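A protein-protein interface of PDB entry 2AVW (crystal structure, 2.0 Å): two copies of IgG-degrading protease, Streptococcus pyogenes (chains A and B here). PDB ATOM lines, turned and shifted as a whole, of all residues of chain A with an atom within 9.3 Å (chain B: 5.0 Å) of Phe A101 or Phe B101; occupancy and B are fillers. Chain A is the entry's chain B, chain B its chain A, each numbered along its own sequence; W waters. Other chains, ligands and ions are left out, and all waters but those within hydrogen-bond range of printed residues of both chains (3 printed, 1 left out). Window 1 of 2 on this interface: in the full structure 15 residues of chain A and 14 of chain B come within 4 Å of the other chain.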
ATOM      1  N   LYS A  98       6.044  21.676 -30.321  1.00  0.00           N
ATOM      2  CA  LYS A  98       7.356  22.191 -30.680  1.00  0.00           C
ATOM      3  C   LYS A  98       7.851  23.394 -29.901  1.00  0.00           C
ATOM      4  O   LYS A  98       7.068  24.160 -29.343  1.00  0.00           O
ATOM      5  CB  LYS A  98       7.381  22.511 -32.174  1.00  0.00           C
ATOM      6  CG  LYS A  98       7.328  21.279 -33.049  1.00  0.00           C
ATOM      7  CD  LYS A  98       7.349  21.648 -34.517  1.00  0.00           C
ATOM      8  CE  LYS A  98       7.453  20.408 -35.396  1.00  0.00           C
ATOM      9  NZ  LYS A  98       7.608  20.774 -36.826  1.00  0.00           N
ATOM     10  N   ILE A  99       9.173  23.529 -29.857  1.00  0.00           N
ATOM     11  CA  ILE A  99       9.820  24.649 -29.195  1.00  0.00           C
ATOM     12  C   ILE A  99      10.542  25.407 -30.300  1.00  0.00           C
ATOM     13  O   ILE A  99      11.462  24.879 -30.930  1.00  0.00           O
ATOM     14  CB  ILE A  99      10.874  24.199 -28.151  1.00  0.00           C
ATOM     15  CG1 ILE A  99      10.195  23.501 -26.965  1.00  0.00           C
ATOM     16  CG2 ILE A  99      11.664  25.409 -27.661  1.00  0.00           C
ATOM     17  CD1 ILE A  99      11.182  23.015 -25.904  1.00  0.00           C
ATOM     18  N   ASN A 100      10.118  26.639 -30.545  1.00  0.00           N
ATOM     19  CA  ASN A 100      10.743  27.444 -31.582  1.00  0.00           C
ATOM     20  C   ASN A 100      11.422  28.675 -31.014  1.00  0.00           C
ATOM     21  O   ASN A 100      10.914  29.321 -30.094  1.00  0.00           O
ATOM     22  CB  ASN A 100       9.714  27.868 -32.635  1.00  0.00           C
ATOM     23  CG  ASN A 100       9.528  26.821 -33.722  1.00  0.00           C
ATOM     24  OD1 ASN A 100       8.965  25.749 -33.485  1.00  0.00           O
ATOM     25  ND2 ASN A 100      10.010  27.128 -34.922  1.00  0.00           N
ATOM     26  N   PHE A 101      12.586  28.986 -31.572  1.00  0.00           N
ATOM     27  CA  PHE A 101      13.348  30.145 -31.148  1.00  0.00           C
ATOM     28  C   PHE A 101      13.562  31.051 -32.352  1.00  0.00           C
ATOM     29  O   PHE A 101      14.286  30.707 -33.293  1.00  0.00           O
ATOM     30  CB  PHE A 101      14.703  29.725 -30.573  1.00  0.00           C
ATOM     31  CG  PHE A 101      15.482  30.858 -29.948  1.00  0.00           C
ATOM     32  CD1 PHE A 101      16.779  30.654 -29.489  1.00  0.00           C
ATOM     33  CD2 PHE A 101      14.922  32.132 -29.818  1.00  0.00           C
ATOM     34  CE1 PHE A 101      17.507  31.697 -28.908  1.00  0.00           C
ATOM     35  CE2 PHE A 101      15.644  33.180 -29.237  1.00  0.00           C
ATOM     36  CZ  PHE A 101      16.936  32.961 -28.785  1.00  0.00           C
ATOM     37  N   ASN A 102      12.904  32.202 -32.312  1.00  0.00           N
ATOM     38  CA  ASN A 102      13.002  33.212 -33.359  1.00  0.00           C
ATOM     39  C   ASN A 102      13.178  32.623 -34.757  1.00  0.00           C
ATOM     40  O   ASN A 102      14.133  32.944 -35.464  1.00  0.00           O
ATOM     41  CB  ASN A 102      14.160  34.159 -33.028  1.00  0.00           C
ATOM     42  CG  ASN A 102      14.231  35.338 -33.966  1.00  0.00           C
ATOM     43  OD1 ASN A 102      13.211  35.963 -34.278  1.00  0.00           O
ATOM     44  ND2 ASN A 102      15.437  35.663 -34.412  1.00  0.00           N
ATOM     45  N   GLY A 103      12.258  31.746 -35.145  1.00  0.00           N
ATOM     46  CA  GLY A 103      12.330  31.147 -36.461  1.00  0.00           C
ATOM     47  C   GLY A 103      12.935  29.760 -36.536  1.00  0.00           C
ATOM     48  O   GLY A 103      12.545  28.969 -37.393  1.00  0.00           O
ATOM     49  N   GLU A 104      13.883  29.450 -35.659  1.00  0.00           N
ATOM     50  CA  GLU A 104      14.515  28.131 -35.679  1.00  0.00           C
ATOM     51  C   GLU A 104      13.843  27.119 -34.751  1.00  0.00           C
ATOM     52  O   GLU A 104      13.591  27.407 -33.584  1.00  0.00           O
ATOM     53  CB  GLU A 104      16.004  28.247 -35.320  1.00  0.00           C
ATOM     54  CG  GLU A 104      16.516  27.087 -34.468  1.00  0.00           C
ATOM     55  CD  GLU A 104      18.021  26.861 -34.561  1.00  0.00           C
ATOM     56  OE1 GLU A 104      18.805  27.802 -34.305  1.00  0.00           O
ATOM     57  OE2 GLU A 104      18.419  25.720 -34.882  1.00  0.00           O
ATOM     58  N   GLN A 105      13.557  25.929 -35.272  1.00  0.00           N
ATOM     59  CA  GLN A 105      12.934  24.889 -34.458  1.00  0.00           C
ATOM     60  C   GLN A 105      14.008  24.217 -33.605  1.00  0.00           C
ATOM     61  O   GLN A 105      14.947  23.606 -34.121  1.00  0.00           O
ATOM     62  CB  GLN A 105      12.239  23.839 -35.324  1.00  0.00           C
ATOM     63  CG  GLN A 105      11.659  22.694 -34.497  1.00  0.00           C
ATOM     64  CD  GLN A 105      10.921  21.669 -35.335  1.00  0.00           C
ATOM     65  OE1 GLN A 105       9.869  21.959 -35.901  1.00  0.00           O
ATOM     66  NE2 GLN A 105      11.475  20.460 -35.419  1.00  0.00           N
ATOM     67  N   MET A 106      13.855  24.343 -32.293  1.00  0.00           N
ATOM     68  CA  MET A 106      14.803  23.785 -31.338  1.00  0.00           C
ATOM     69  C   MET A 106      14.443  22.365 -30.933  1.00  0.00           C
ATOM     70  O   MET A 106      15.319  21.526 -30.698  1.00  0.00           O
ATOM     71  CB  MET A 106      14.830  24.661 -30.084  1.00  0.00           C
ATOM     72  CG  MET A 106      15.156  26.118 -30.350  1.00  0.00           C
ATOM     73  SD  MET A 106      16.921  26.403 -30.471  1.00  0.00           S
ATOM     74  CE  MET A 106      17.347  25.457 -31.903  1.00  0.00           C
ATOM     75  N   PHE A 107      13.145  22.100 -30.853  1.00  0.00           N
ATOM     76  CA  PHE A 107      12.680  20.791 -30.421  1.00  0.00           C
ATOM     77  C   PHE A 107      11.253  20.503 -30.862  1.00  0.00           C
ATOM     78  O   PHE A 107      10.437  21.418 -31.010  1.00  0.00           O
ATOM     79  CB  PHE A 107      12.758  20.723 -28.896  1.00  0.00           C
ATOM     80  CG  PHE A 107      12.459  19.367 -28.318  1.00  0.00           C
ATOM     81  CD1 PHE A 107      13.322  18.293 -28.532  1.00  0.00           C
ATOM     82  CD2 PHE A 107      11.336  19.176 -27.522  1.00  0.00           C
ATOM     83  CE1 PHE A 107      13.072  17.043 -27.951  1.00  0.00           C
ATOM     84  CE2 PHE A 107      11.077  17.929 -26.936  1.00  0.00           C
ATOM     85  CZ  PHE A 107      11.948  16.864 -27.151  1.00  0.00           C
ATOM     86  N   TYR A 127      18.712  17.473 -27.917  1.00  0.00           N
ATOM     87  CA  TYR A 127      18.163  18.758 -27.514  1.00  0.00           C
ATOM     88  C   TYR A 127      18.847  19.243 -26.236  1.00  0.00           C
ATOM     89  O   TYR A 127      19.163  20.437 -26.095  1.00  0.00           O
ATOM     90  CB  TYR A 127      16.655  18.645 -27.270  1.00  0.00           C
ATOM     91  CG  TYR A 127      16.056  19.900 -26.678  1.00  0.00           C
ATOM     92  CD1 TYR A 127      16.156  21.115 -27.346  1.00  0.00           C
ATOM     93  CD2 TYR A 127      15.418  19.881 -25.440  1.00  0.00           C
ATOM     94  CE1 TYR A 127      15.645  22.287 -26.801  1.00  0.00           C
ATOM     95  CE2 TYR A 127      14.896  21.051 -24.881  1.00  0.00           C
ATOM     96  CZ  TYR A 127      15.017  22.254 -25.575  1.00  0.00           C
ATOM     97  OH  TYR A 127      14.517  23.420 -25.053  1.00  0.00           O
ATOM     98  N   LYS A 131      21.017  22.356 -27.400  1.00  0.00           N
ATOM     99  CA  LYS A 131      20.220  23.568 -27.237  1.00  0.00           C
ATOM    100  C   LYS A 131      19.900  24.000 -25.810  1.00  0.00           C
ATOM    101  O   LYS A 131      19.935  25.192 -25.491  1.00  0.00           O
ATOM    102  CB  LYS A 131      18.901  23.406 -27.997  1.00  0.00           C
ATOM    103  CG  LYS A 131      19.047  22.832 -29.400  1.00  0.00           C
ATOM    104  CD  LYS A 131      19.773  23.779 -30.326  1.00  0.00           C
ATOM    105  CE  LYS A 131      19.862  23.200 -31.729  1.00  0.00           C
ATOM    106  NZ  LYS A 131      20.579  24.114 -32.655  1.00  0.00           N
ATOM    107  N   ALA A 132      19.574  23.034 -24.959  1.00  0.00           N
ATOM    108  CA  ALA A 132      19.207  23.323 -23.576  1.00  0.00           C
ATOM    109  C   ALA A 132      20.370  23.613 -22.635  1.00  0.00           C
ATOM    110  O   ALA A 132      20.359  24.613 -21.916  1.00  0.00           O
ATOM    111  CB  ALA A 132      18.378  22.174 -23.019  1.00  0.00           C
ATOM    112  N   MET A 151      11.936  21.234 -15.415  1.00  0.00           N
ATOM    113  CA  MET A 151      11.981  22.234 -16.481  1.00  0.00           C
ATOM    114  C   MET A 151      11.226  21.760 -17.715  1.00  0.00           C
ATOM    115  O   MET A 151      10.329  22.434 -18.210  1.00  0.00           O
ATOM    116  CB  MET A 151      13.425  22.521 -16.891  1.00  0.00           C
ATOM    117  CG  MET A 151      13.518  23.446 -18.097  1.00  0.00           C
ATOM    118  SD  MET A 151      15.130  23.400 -18.866  1.00  0.00           S
ATOM    119  CE  MET A 151      14.935  21.984 -19.992  1.00  0.00           C
ATOM    120  N   ARG A 157      11.802  27.244 -14.319  1.00  0.00           N
ATOM    121  CA  ARG A 157      13.020  27.838 -14.835  1.00  0.00           C
ATOM    122  C   ARG A 157      14.183  27.195 -14.107  1.00  0.00           C
ATOM    123  O   ARG A 157      14.293  27.280 -12.888  1.00  0.00           O
ATOM    124  CB  ARG A 157      13.015  29.356 -14.614  1.00  0.00           C
ATOM    125  CG  ARG A 157      11.827  30.075 -15.257  1.00  0.00           C
ATOM    126  CD  ARG A 157      11.935  31.597 -15.124  1.00  0.00           C
ATOM    127  NE  ARG A 157      12.749  32.205 -16.176  1.00  0.00           N
ATOM    128  CZ  ARG A 157      12.337  32.419 -17.425  1.00  0.00           C
ATOM    129  NH1 ARG A 157      11.111  32.080 -17.792  1.00  0.00           N
ATOM    130  NH2 ARG A 157      13.154  32.972 -18.309  1.00  0.00           N
ATOM    131  N   LYS A 173       7.421  30.523 -17.344  1.00  0.00           N
ATOM    132  CA  LYS A 173       7.895  29.249 -17.857  1.00  0.00           C
ATOM    133  C   LYS A 173       9.280  29.360 -18.490  1.00  0.00           C
ATOM    134  O   LYS A 173       9.620  30.386 -19.082  1.00  0.00           O
ATOM    135  CB  LYS A 173       6.894  28.721 -18.882  1.00  0.00           C
ATOM    136  CG  LYS A 173       7.452  27.688 -19.827  1.00  0.00           C
ATOM    137  CD  LYS A 173       6.377  27.172 -20.749  1.00  0.00           C
ATOM    138  CE  LYS A 173       6.866  27.108 -22.182  1.00  0.00           C
ATOM    139  NZ  LYS A 173       6.782  28.408 -22.886  1.00  0.00           N
ATOM    140  N   ASP A 174      10.083  28.305 -18.354  1.00  0.00           N
ATOM    141  CA  ASP A 174      11.417  28.288 -18.956  1.00  0.00           C
ATOM    142  C   ASP A 174      11.197  28.024 -20.439  1.00  0.00           C
ATOM    143  O   ASP A 174      10.559  27.040 -20.808  1.00  0.00           O
ATOM    144  CB  ASP A 174      12.283  27.166 -18.364  1.00  0.00           C
ATOM    145  CG  ASP A 174      13.755  27.275 -18.769  1.00  0.00           C
ATOM    146  OD1 ASP A 174      14.049  27.387 -19.981  1.00  0.00           O
ATOM    147  OD2 ASP A 174      14.624  27.245 -17.866  1.00  0.00           O
ATOM    148  N   PRO A 175      11.709  28.914 -21.306  1.00  0.00           N
ATOM    149  CA  PRO A 175      11.577  28.788 -22.763  1.00  0.00           C
ATOM    150  C   PRO A 175      12.021  27.426 -23.277  1.00  0.00           C
ATOM    151  O   PRO A 175      11.518  26.939 -24.290  1.00  0.00           O
ATOM    152  CB  PRO A 175      12.478  29.903 -23.290  1.00  0.00           C
ATOM    153  CG  PRO A 175      12.370  30.943 -22.247  1.00  0.00           C
ATOM    154  CD  PRO A 175      12.413  30.162 -20.950  1.00  0.00           C
ATOM    155  N   ARG A 176      12.972  26.820 -22.574  1.00  0.00           N
ATOM    156  CA  ARG A 176      13.498  25.518 -22.955  1.00  0.00           C
ATOM    157  C   ARG A 176      12.581  24.348 -22.622  1.00  0.00           C
ATOM    158  O   ARG A 176      12.832  23.234 -23.067  1.00  0.00           O
ATOM    159  CB  ARG A 176      14.850  25.282 -22.285  1.00  0.00           C
ATOM    160  CG  ARG A 176      15.939  26.235 -22.736  1.00  0.00           C
ATOM    161  CD  ARG A 176      17.155  26.134 -21.839  1.00  0.00           C
ATOM    162  NE  ARG A 176      16.830  26.532 -20.474  1.00  0.00           N
ATOM    163  CZ  ARG A 176      17.720  26.643 -19.495  1.00  0.00           C
ATOM    164  NH1 ARG A 176      19.001  26.377 -19.731  1.00  0.00           N
ATOM    165  NH2 ARG A 176      17.330  27.042 -18.289  1.00  0.00           N
ATOM    166  N   GLY A 177      11.526  24.589 -21.849  1.00  0.00           N
ATOM    167  CA  GLY A 177      10.635  23.490 -21.501  1.00  0.00           C
ATOM    168  C   GLY A 177       9.169  23.843 -21.315  1.00  0.00           C
ATOM    169  O   GLY A 177       8.600  24.605 -22.099  1.00  0.00           O
ATOM    170  N   ILE B  99      12.102  39.170 -31.308  1.00  0.00           N
ATOM    171  CA  ILE B  99      12.754  37.870 -31.197  1.00  0.00           C
ATOM    172  C   ILE B  99      11.984  37.108 -30.121  1.00  0.00           C
ATOM    173  O   ILE B  99      12.012  37.487 -28.949  1.00  0.00           O
ATOM    174  CB  ILE B  99      14.240  37.994 -30.768  1.00  0.00           C
ATOM    175  CG1 ILE B  99      15.032  38.757 -31.834  1.00  0.00           C
ATOM    176  CG2 ILE B  99      14.847  36.601 -30.566  1.00  0.00           C
ATOM    177  CD1 ILE B  99      16.506  38.879 -31.520  1.00  0.00           C
ATOM    178  N   ASN B 100      11.286  36.052 -30.528  1.00  0.00           N
ATOM    179  CA  ASN B 100      10.496  35.252 -29.596  1.00  0.00           C
ATOM    180  C   ASN B 100      11.092  33.868 -29.368  1.00  0.00           C
ATOM    181  O   ASN B 100      11.588  33.235 -30.295  1.00  0.00           O
ATOM    182  CB  ASN B 100       9.059  35.100 -30.114  1.00  0.00           C
ATOM    183  CG  ASN B 100       8.300  36.417 -30.139  1.00  0.00           C
ATOM    184  OD1 ASN B 100       8.233  37.128 -29.134  1.00  0.00           O
ATOM    185  ND2 ASN B 100       7.716  36.745 -31.291  1.00  0.00           N
ATOM    186  N   PHE B 101      11.047  33.404 -28.121  1.00  0.00           N
ATOM    187  CA  PHE B 101      11.568  32.088 -27.796  1.00  0.00           C
ATOM    188  C   PHE B 101      10.484  31.285 -27.091  1.00  0.00           C
ATOM    189  O   PHE B 101      10.162  31.528 -25.924  1.00  0.00           O
ATOM    190  CB  PHE B 101      12.811  32.178 -26.902  1.00  0.00           C
ATOM    191  CG  PHE B 101      13.502  30.850 -26.680  1.00  0.00           C
ATOM    192  CD1 PHE B 101      14.551  30.743 -25.771  1.00  0.00           C
ATOM    193  CD2 PHE B 101      13.109  29.708 -27.384  1.00  0.00           C
ATOM    194  CE1 PHE B 101      15.202  29.511 -25.566  1.00  0.00           C
ATOM    195  CE2 PHE B 101      13.748  28.479 -27.186  1.00  0.00           C
ATOM    196  CZ  PHE B 101      14.797  28.379 -26.276  1.00  0.00           C
ATOM    197  N   ASN B 102       9.914  30.344 -27.833  1.00  0.00           N
ATOM    198  CA  ASN B 102       8.868  29.468 -27.337  1.00  0.00           C
ATOM    199  C   ASN B 102       7.840  30.202 -26.476  1.00  0.00           C
ATOM    200  O   ASN B 102       7.577  29.821 -25.331  1.00  0.00           O
ATOM    201  CB  ASN B 102       9.508  28.310 -26.564  1.00  0.00           C
ATOM    202  CG  ASN B 102       8.487  27.312 -26.048  1.00  0.00           C
ATOM    203  OD1 ASN B 102       7.448  27.094 -26.668  1.00  0.00           O
ATOM    204  ND2 ASN B 102       8.791  26.685 -24.918  1.00  0.00           N
ATOM    205  N   GLY B 103       7.268  31.267 -27.033  1.00  0.00           N
ATOM    206  CA  GLY B 103       6.253  32.017 -26.316  1.00  0.00           C
ATOM    207  C   GLY B 103       6.699  33.196 -25.476  1.00  0.00           C
ATOM    208  O   GLY B 103       5.860  33.929 -24.945  1.00  0.00           O
ATOM    209  N   GLU B 104       8.004  33.390 -25.341  1.00  0.00           N
ATOM    210  CA  GLU B 104       8.512  34.502 -24.551  1.00  0.00           C
ATOM    211  C   GLU B 104       9.250  35.494 -25.450  1.00  0.00           C
ATOM    212  O   GLU B 104      10.027  35.094 -26.324  1.00  0.00           O
ATOM    213  CB  GLU B 104       9.456  33.989 -23.457  1.00  0.00           C
ATOM    214  CG  GLU B 104      10.066  35.094 -22.600  1.00  0.00           C
ATOM    215  CD  GLU B 104      11.058  34.576 -21.559  1.00  0.00           C
ATOM    216  OE1 GLU B 104      11.756  35.418 -20.950  1.00  0.00           O
ATOM    217  OE2 GLU B 104      11.136  33.343 -21.346  1.00  0.00           O
ATOM    218  N   GLN B 105       8.994  36.785 -25.241  1.00  0.00           N
ATOM    219  CA  GLN B 105       9.651  37.814 -26.035  1.00  0.00           C
ATOM    220  C   GLN B 105      11.014  38.105 -25.428  1.00  0.00           C
ATOM    221  O   GLN B 105      11.121  38.522 -24.274  1.00  0.00           O
ATOM    222  CB  GLN B 105       8.813  39.096 -26.088  1.00  0.00           C
ATOM    223  CG  GLN B 105       9.469  40.206 -26.918  1.00  0.00           C
ATOM    224  CD  GLN B 105       8.578  41.420 -27.096  1.00  0.00           C
ATOM    225  OE1 GLN B 105       7.503  41.334 -27.698  1.00  0.00           O
ATOM    226  NE2 GLN B 105       9.021  42.564 -26.574  1.00  0.00           N
ATOM    227  N   MET B 106      12.056  37.862 -26.213  1.00  0.00           N
ATOM    228  CA  MET B 106      13.431  38.072 -25.771  1.00  0.00           C
ATOM    229  C   MET B 106      13.929  39.468 -26.113  1.00  0.00           C
ATOM    230  O   MET B 106      14.735  40.044 -25.377  1.00  0.00           O
ATOM    231  CB  MET B 106      14.351  37.058 -26.451  1.00  0.00           C
ATOM    232  CG  MET B 106      13.885  35.608 -26.392  1.00  0.00           C
ATOM    233  SD  MET B 106      14.147  34.841 -24.776  1.00  0.00           S
ATOM    234  CE  MET B 106      12.834  35.538 -23.892  1.00  0.00           C
ATOM    235  N   PRO B 175      19.574  32.204 -33.841  1.00  0.00           N
ATOM    236  CA  PRO B 175      18.267  32.590 -33.299  1.00  0.00           C
ATOM    237  C   PRO B 175      18.316  33.897 -32.508  1.00  0.00           C
ATOM    238  O   PRO B 175      17.302  34.560 -32.333  1.00  0.00           O
ATOM    239  CB  PRO B 175      17.903  31.412 -32.391  1.00  0.00           C
ATOM    240  CG  PRO B 175      18.639  30.264 -32.983  1.00  0.00           C
ATOM    241  CD  PRO B 175      19.958  30.860 -33.373  1.00  0.00           C
ATOM    242  N   ARG B 176      19.501  34.259 -32.030  1.00  0.00           N
ATOM    243  CA  ARG B 176      19.672  35.475 -31.237  1.00  0.00           C
ATOM    244  C   ARG B 176      19.794  36.770 -32.040  1.00  0.00           C
ATOM    245  O   ARG B 176      19.820  37.862 -31.463  1.00  0.00           O
ATOM    246  CB  ARG B 176      20.894  35.334 -30.326  1.00  0.00           C
ATOM    247  CG  ARG B 176      20.757  34.262 -29.265  1.00  0.00           C
ATOM    248  CD  ARG B 176      22.064  34.021 -28.545  1.00  0.00           C
ATOM    249  NE  ARG B 176      23.093  33.523 -29.452  1.00  0.00           N
ATOM    250  CZ  ARG B 176      24.326  33.197 -29.076  1.00  0.00           C
ATOM    251  NH1 ARG B 176      24.682  33.317 -27.796  1.00  0.00           N
ATOM    252  NH2 ARG B 176      25.199  32.747 -29.971  1.00  0.00           N
HETATM  253  O   HOH W   1       7.649  27.457 -29.659  1.00  0.00           O
HETATM  254  O   HOH W   2      14.174  33.446 -20.917  1.00  0.00           O
HETATM  255  O   HOH W   3      10.703  35.783 -33.248  1.00  0.00           O
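Of the 10 printed residues of chain B, 6 touch a printed residue of chain A. Printed residues of chain B that touch a printed residue of chain A: Ile B99, Asn B100, Phe B101, Asn B102, Glu B104 and Pro B175. Hydrophobic or aromatic side chains of chain B within 4 Å of the printed part of chain A: Ile B99, Phe B101 and Pro B175. Hydrophobic or aromatic side chains of chain A within 4 Å of the printed part of chain B: Ile A99, Phe A101 and Pro A175. Among the printed residues, 20 pairs touch across the chains.
The backbone NH (N) of Asn A102 lies within hydrogen-bond range of the backbone carbonyl oxygen (O) of Asn B100. N of Asn B102 sits at hydrogen-bond distance from O of Asn A100. NZ of Lys A173 lies within hydrogen-bond range of O of Asn B102 (2.9 Å). The side-chain amide nitrogen of Asn B102 sits at hydrogen-bond distance from the backbone carbonyl oxygen of Pro A175, at 2.8 Å. The side-chain carboxylate (OE2) of Glu B104 lies within salt-bridge range of the guanidinium group (NH2) of Arg A157 (3.7 Å). The side-chain amide nitrogen (ND2) of Asn A102 sits at hydrogen-bond distance from the backbone carbonyl oxygen (O) of Pro B175 (3.0 Å).
Ile A99 touches Asn B102 (CG2 to CB, 3.8 Å). Asn B100 touches Asn A100. Asn A100 touches Phe B101 (O to CD2, 3.5 Å). Phe A101 touches Ile B99. Phe A101 touches Asn B100 (CD2 to O, 3.5 Å). CB of Phe A101 touches CD2 of Phe B101, at 3.6 Å. Pro B175 touches Phe A101 (CB to CD1, 3.2 Å). Asn A102 touches Ile B99. Phe B101 touches Pro A175. Glu B104 touches Pro A175 (OE2 to CG, 2.8 Å).
Ile A99 touches Phe B101, and with the chains exchanged Phe A101 touches Ile B99. Ile A99 touches Asn B102, and with the chains exchanged Asn A102 touches Ile B99. Asn A100 touches its own counterpart, Asn B100. Asn A100 touches Phe B101, and with the chains exchanged Phe A101 touches Asn B100. 10 positions are printed for both chains. Of the 20 pairs that touch across the chains among the printed residues, 16 have their exchanged pair printed and touching as well.
The backbone NH (N) of Met B106 sits at hydrogen-bond distance from the backbone carbonyl oxygen (O) of Ile B99 (2.8 Å). The side-chain amino group (NZ) of Lys A98 sits at hydrogen-bond distance from the side-chain amide oxygen (OE1) of Gln A105 (2.7 Å). The backbone carbonyl oxygen (O) of Ile A99 lies within hydrogen-bond range of the backbone NH (N) of Met A106, at 2.8 Å. The backbone carbonyl oxygen (O) of Phe A107 sits at hydrogen-bond distance from the backbone NH (N) of Ile A99, at 2.7 Å. OE2 of Glu A104 lies within salt-bridge range of NZ of Lys A131, 3.5 Å away. The backbone carbonyl oxygen of Lys A173 is in hydrogen-bond range of the guanidinium group of Arg A157, 2.6 Å away.
Water W3 bridges the side-chain amide oxygen of Asn A102 and the backbone NH of Asn B100. Water W1 lies within hydrogen-bond range of N of Asn A100, OD1 of Asn B102 and O of Lys A98. Water W2 bridges NH2 of Arg A157 (2.8 Å) and OE2 of Glu B104 (3.1 Å).
Of chain B, only Ile B99 (3.8 Å), Asn B100 (3.5 Å), Phe B101 (3.6 Å) and Pro B175 (3.2 Å) come within 4 Å of Phe A101. Phe B101 touches just these residues of chain A: Ile A99 (3.7 Å), Asn A100 (3.5 Å), Phe A101 (3.6 Å) and Pro A175 (3.3 Å). No residue of chain A comes within 4 Å of Gly B103. Printed residues of chain B within 4 Å of Arg A157: Glu B104 (3.7 Å). Of the printed residues of chain A, Glu B104 touches Arg A157 (3.7 Å) and Pro A175 (2.8 Å). Printed residues of chain B within 4 Å of Pro A175: Phe B101 (3.3 Å), Asn B102 (2.8 Å) and Glu B104 (2.8 Å). Of the printed residues of chain B, Gly A177 touches Asn B102 (3.5 Å). Of the printed residues of chain A, Ile B99 touches Phe A101 and Asn A102. Gln A105 touches none of the printed residues of chain B. Met A151 touches none of the printed residues of chain B. The nearest printed residue of chain B that does not touch Ile A99 is Gly B103 (7.4 Å).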
